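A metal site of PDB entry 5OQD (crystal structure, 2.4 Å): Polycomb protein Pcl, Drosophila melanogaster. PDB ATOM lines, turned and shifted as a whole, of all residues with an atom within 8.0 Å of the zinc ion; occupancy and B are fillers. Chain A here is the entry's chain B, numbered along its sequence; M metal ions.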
ATOM      1  N   GLN A  44     -21.146  19.121 -23.814  1.00  0.00           N
ATOM      2  CA  GLN A  44     -19.721  19.068 -24.149  1.00  0.00           C
ATOM      3  C   GLN A  44     -19.516  19.297 -25.646  1.00  0.00           C
ATOM      4  O   GLN A  44     -20.194  18.675 -26.471  1.00  0.00           O
ATOM      5  CB  GLN A  44     -19.110  17.732 -23.729  1.00  0.00           C
ATOM      6  CG  GLN A  44     -17.612  17.649 -23.927  1.00  0.00           C
ATOM      7  CD  GLN A  44     -17.051  16.291 -23.533  1.00  0.00           C
ATOM      8  OE1 GLN A  44     -17.752  15.284 -23.561  1.00  0.00           O
ATOM      9  NE2 GLN A  44     -15.778  16.277 -23.147  1.00  0.00           N
ATOM     10  N   CYS A  45     -18.592  20.188 -25.996  1.00  0.00           N
ATOM     11  CA  CYS A  45     -18.289  20.458 -27.394  1.00  0.00           C
ATOM     12  C   CYS A  45     -17.640  19.231 -28.030  1.00  0.00           C
ATOM     13  O   CYS A  45     -16.762  18.596 -27.443  1.00  0.00           O
ATOM     14  CB  CYS A  45     -17.369  21.668 -27.517  1.00  0.00           C
ATOM     15  SG  CYS A  45     -16.894  22.089 -29.219  1.00  0.00           S
ATOM     16  N   CYS A  46     -18.079  18.879 -29.223  1.00  0.00           N
ATOM     17  CA  CYS A  46     -17.456  17.771 -29.926  1.00  0.00           C
ATOM     18  C   CYS A  46     -16.003  17.984 -30.340  1.00  0.00           C
ATOM     19  O   CYS A  46     -15.230  17.055 -30.310  1.00  0.00           O
ATOM     20  CB  CYS A  46     -18.326  17.266 -31.084  1.00  0.00           C
ATOM     21  SG  CYS A  46     -18.773  18.460 -32.338  1.00  0.00           S
ATOM     22  N   LYS A  47     -15.652  19.168 -30.824  1.00  0.00           N
ATOM     23  CA  LYS A  47     -14.247  19.473 -31.109  1.00  0.00           C
ATOM     24  C   LYS A  47     -13.210  19.739 -29.993  1.00  0.00           C
ATOM     25  O   LYS A  47     -12.152  19.143 -29.993  1.00  0.00           O
ATOM     26  CB  LYS A  47     -14.182  20.540 -32.207  1.00  0.00           C
ATOM     27  CG  LYS A  47     -14.801  20.057 -33.500  1.00  0.00           C
ATOM     28  CD  LYS A  47     -14.806  21.125 -34.574  1.00  0.00           C
ATOM     29  CE  LYS A  47     -14.519  20.530 -35.930  1.00  0.00           C
ATOM     30  NZ  LYS A  47     -15.005  21.399 -37.024  1.00  0.00           N
ATOM     31  N   CYS A  48     -13.538  20.584 -29.024  1.00  0.00           N
ATOM     32  CA  CYS A  48     -12.606  20.978 -27.971  1.00  0.00           C
ATOM     33  C   CYS A  48     -12.822  20.167 -26.702  1.00  0.00           C
ATOM     34  O   CYS A  48     -11.959  20.134 -25.815  1.00  0.00           O
ATOM     35  CB  CYS A  48     -12.740  22.472 -27.676  1.00  0.00           C
ATOM     36  SG  CYS A  48     -14.321  22.982 -26.959  1.00  0.00           S
ATOM     37  N   ARG A  49     -13.974  19.508 -26.624  1.00  0.00           N
ATOM     38  CA  ARG A  49     -14.322  18.594 -25.530  1.00  0.00           C
ATOM     39  C   ARG A  49     -14.420  19.302 -24.169  1.00  0.00           C
ATOM     40  O   ARG A  49     -14.309  18.653 -23.122  1.00  0.00           O
ATOM     41  CB  ARG A  49     -13.313  17.441 -25.459  1.00  0.00           C
ATOM     42  CG  ARG A  49     -13.066  16.783 -26.808  1.00  0.00           C
ATOM     43  CD  ARG A  49     -12.073  15.651 -26.724  1.00  0.00           C
ATOM     44  NE  ARG A  49     -11.695  15.187 -28.066  1.00  0.00           N
ATOM     45  CZ  ARG A  49     -10.801  14.237 -28.307  1.00  0.00           C
ATOM     46  NH1 ARG A  49     -10.193  13.636 -27.290  1.00  0.00           N
ATOM     47  NH2 ARG A  49     -10.513  13.896 -29.549  1.00  0.00           N
ATOM     48  N   ASN A  50     -14.636  20.611 -24.195  1.00  0.00           N
ATOM     49  CA  ASN A  50     -14.906  21.365 -22.986  1.00  0.00           C
ATOM     50  C   ASN A  50     -16.409  21.377 -22.703  1.00  0.00           C
ATOM     51  O   ASN A  50     -17.217  21.176 -23.595  1.00  0.00           O
ATOM     52  CB  ASN A  50     -14.378  22.790 -23.100  1.00  0.00           C
ATOM     53  CG  ASN A  50     -12.874  22.862 -23.021  1.00  0.00           C
ATOM     54  OD1 ASN A  50     -12.235  22.155 -22.225  1.00  0.00           O
ATOM     55  ND2 ASN A  50     -12.266  23.709 -23.845  1.00  0.00           N
ATOM     56  N   TRP A  51     -16.772  21.622 -21.441  1.00  0.00           N
ATOM     57  CA  TRP A  51     -18.172  21.663 -21.055  1.00  0.00           C
ATOM     58  C   TRP A  51     -18.680  23.101 -20.992  1.00  0.00           C
ATOM     59  O   TRP A  51     -17.947  24.016 -20.620  1.00  0.00           O
ATOM     60  CB  TRP A  51     -18.392  20.950 -19.723  1.00  0.00           C
ATOM     61  CG  TRP A  51     -18.068  19.493 -19.777  1.00  0.00           C
ATOM     62  CD1 TRP A  51     -16.848  18.911 -19.623  1.00  0.00           C
ATOM     63  CD2 TRP A  51     -18.986  18.409 -20.012  1.00  0.00           C
ATOM     64  NE1 TRP A  51     -16.945  17.552 -19.742  1.00  0.00           N
ATOM     65  CE2 TRP A  51     -18.249  17.216 -19.985  1.00  0.00           C
ATOM     66  CE3 TRP A  51     -20.367  18.345 -20.248  1.00  0.00           C
ATOM     67  CZ2 TRP A  51     -18.838  15.973 -20.171  1.00  0.00           C
ATOM     68  CZ3 TRP A  51     -20.947  17.113 -20.440  1.00  0.00           C
ATOM     69  CH2 TRP A  51     -20.190  15.940 -20.399  1.00  0.00           C
ATOM     70  N   PHE A  52     -19.946  23.291 -21.361  1.00  0.00           N
ATOM     71  CA  PHE A  52     -20.525  24.617 -21.431  1.00  0.00           C
ATOM     72  C   PHE A  52     -21.883  24.679 -20.734  1.00  0.00           C
ATOM     73  O   PHE A  52     -22.692  23.764 -20.860  1.00  0.00           O
ATOM     74  CB  PHE A  52     -20.703  25.055 -22.899  1.00  0.00           C
ATOM     75  CG  PHE A  52     -19.406  25.225 -23.640  1.00  0.00           C
ATOM     76  CD1 PHE A  52     -18.702  24.126 -24.122  1.00  0.00           C
ATOM     77  CD2 PHE A  52     -18.900  26.488 -23.881  1.00  0.00           C
ATOM     78  CE1 PHE A  52     -17.525  24.292 -24.821  1.00  0.00           C
ATOM     79  CE2 PHE A  52     -17.715  26.658 -24.577  1.00  0.00           C
ATOM     80  CZ  PHE A  52     -17.024  25.556 -25.049  1.00  0.00           C
ATOM     81  N   PHE A  73     -23.084  19.069 -30.088  1.00  0.00           N
ATOM     82  CA  PHE A  73     -22.774  20.480 -29.907  1.00  0.00           C
ATOM     83  C   PHE A  73     -21.341  20.835 -30.279  1.00  0.00           C
ATOM     84  O   PHE A  73     -20.402  20.121 -29.941  1.00  0.00           O
ATOM     85  CB  PHE A  73     -23.043  20.889 -28.455  1.00  0.00           C
ATOM     86  CG  PHE A  73     -22.545  22.252 -28.099  1.00  0.00           C
ATOM     87  CD1 PHE A  73     -23.007  23.370 -28.774  1.00  0.00           C
ATOM     88  CD2 PHE A  73     -21.604  22.418 -27.097  1.00  0.00           C
ATOM     89  CE1 PHE A  73     -22.538  24.631 -28.448  1.00  0.00           C
ATOM     90  CE2 PHE A  73     -21.135  23.679 -26.771  1.00  0.00           C
ATOM     91  CZ  PHE A  73     -21.599  24.784 -27.453  1.00  0.00           C
ATOM     92  N   CYS A  74     -21.192  21.948 -30.989  1.00  0.00           N
ATOM     93  CA  CYS A  74     -19.879  22.505 -31.294  1.00  0.00           C
ATOM     94  C   CYS A  74     -19.891  23.995 -30.999  1.00  0.00           C
ATOM     95  O   CYS A  74     -20.714  24.740 -31.539  1.00  0.00           O
ATOM     96  CB  CYS A  74     -19.496  22.240 -32.747  1.00  0.00           C
ATOM     97  SG  CYS A  74     -17.773  22.598 -33.133  1.00  0.00           S
ATOM     98  N   CYS A  75     -18.984  24.423 -30.126  1.00  0.00           N
ATOM     99  CA  CYS A  75     -18.977  25.807 -29.661  1.00  0.00           C
ATOM    100  C   CYS A  75     -18.523  26.784 -30.748  1.00  0.00           C
ATOM    101  O   CYS A  75     -18.044  26.359 -31.803  1.00  0.00           O
ATOM    102  CB  CYS A  75     -18.074  25.957 -28.432  1.00  0.00           C
ATOM    103  SG  CYS A  75     -16.307  25.799 -28.767  1.00  0.00           S
ATOM    104  N   THR A  76     -18.669  28.068 -30.468  1.00  0.00           N
ATOM    105  CA  THR A  76     -18.348  29.118 -31.429  1.00  0.00           C
ATOM    106  C   THR A  76     -16.842  29.224 -31.697  1.00  0.00           C
ATOM    107  O   THR A  76     -16.423  29.758 -32.723  1.00  0.00           O
ATOM    108  CB  THR A  76     -18.857  30.481 -30.953  1.00  0.00           C
ATOM    109  OG1 THR A  76     -18.349  30.755 -29.642  1.00  0.00           O
ATOM    110  CG2 THR A  76     -20.378  30.483 -30.902  1.00  0.00           C
ATOM    111  N   VAL A  77     -16.034  28.728 -30.762  1.00  0.00           N
ATOM    112  CA  VAL A  77     -14.581  28.767 -30.919  1.00  0.00           C
ATOM    113  C   VAL A  77     -14.107  27.738 -31.954  1.00  0.00           C
ATOM    114  O   VAL A  77     -13.215  28.021 -32.763  1.00  0.00           O
ATOM    115  CB  VAL A  77     -13.862  28.499 -29.581  1.00  0.00           C
ATOM    116  CG1 VAL A  77     -12.347  28.567 -29.753  1.00  0.00           C
ATOM    117  CG2 VAL A  77     -14.326  29.492 -28.520  1.00  0.00           C
ATOM    118  N   CYS A  78     -14.712  26.558 -31.924  1.00  0.00           N
ATOM    119  CA  CYS A  78     -14.299  25.462 -32.790  1.00  0.00           C
ATOM    120  C   CYS A  78     -15.012  25.464 -34.143  1.00  0.00           C
ATOM    121  O   CYS A  78     -14.613  24.738 -35.059  1.00  0.00           O
ATOM    122  CB  CYS A  78     -14.550  24.120 -32.084  1.00  0.00           C
ATOM    123  SG  CYS A  78     -13.693  23.916 -30.500  1.00  0.00           S
ATOM    124  N   ASN A  79     -16.056  26.273 -34.267  1.00  0.00           N
ATOM    125  CA  ASN A  79     -16.873  26.267 -35.486  1.00  0.00           C
ATOM    126  C   ASN A  79     -16.961  27.639 -36.157  1.00  0.00           C
ATOM    127  O   ASN A  79     -18.019  28.030 -36.642  1.00  0.00           O
ATOM    128  CB  ASN A  79     -18.274  25.738 -35.177  1.00  0.00           C
ATOM    129  CG  ASN A  79     -19.010  25.257 -36.412  1.00  0.00           C
ATOM    130  OD1 ASN A  79     -18.413  24.700 -37.334  1.00  0.00           O
ATOM    131  ND2 ASN A  79     -20.314  25.491 -36.445  1.00  0.00           N
HETATM  132 ZN    ZN M   1     -15.293  23.771 -28.861  1.00  0.00          ZN
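The backbone NH (N) of Asn 50 lies close to the side-chain sulfur (SG) of Cys 48 (3.7 Å). N of Lys 47 sits close to SG of Cys 45, at 3.6 Å. SG of Cys 75 sits close to N of Val 77. N of Cys 45 is in hydrogen-bond range of O of Asn 50.
Within 4 Å of the zinc ion: Cys 45, Cys 48, Cys 75 and Cys 78. The nearest printed residue that does not touch the zinc ion is Phe 52 (4.6 Å).
The zinc ion is bound by the side-chain sulfur of Cys 75 (2.3 Å), the side-chain sulfur of Cys 48 (2.3 Å), the side-chain sulfur of Cys 78 (2.3 Å) and the side-chain sulfur of Cys 45 (2.3 Å). The zinc ion has four donor atoms within binding distance.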
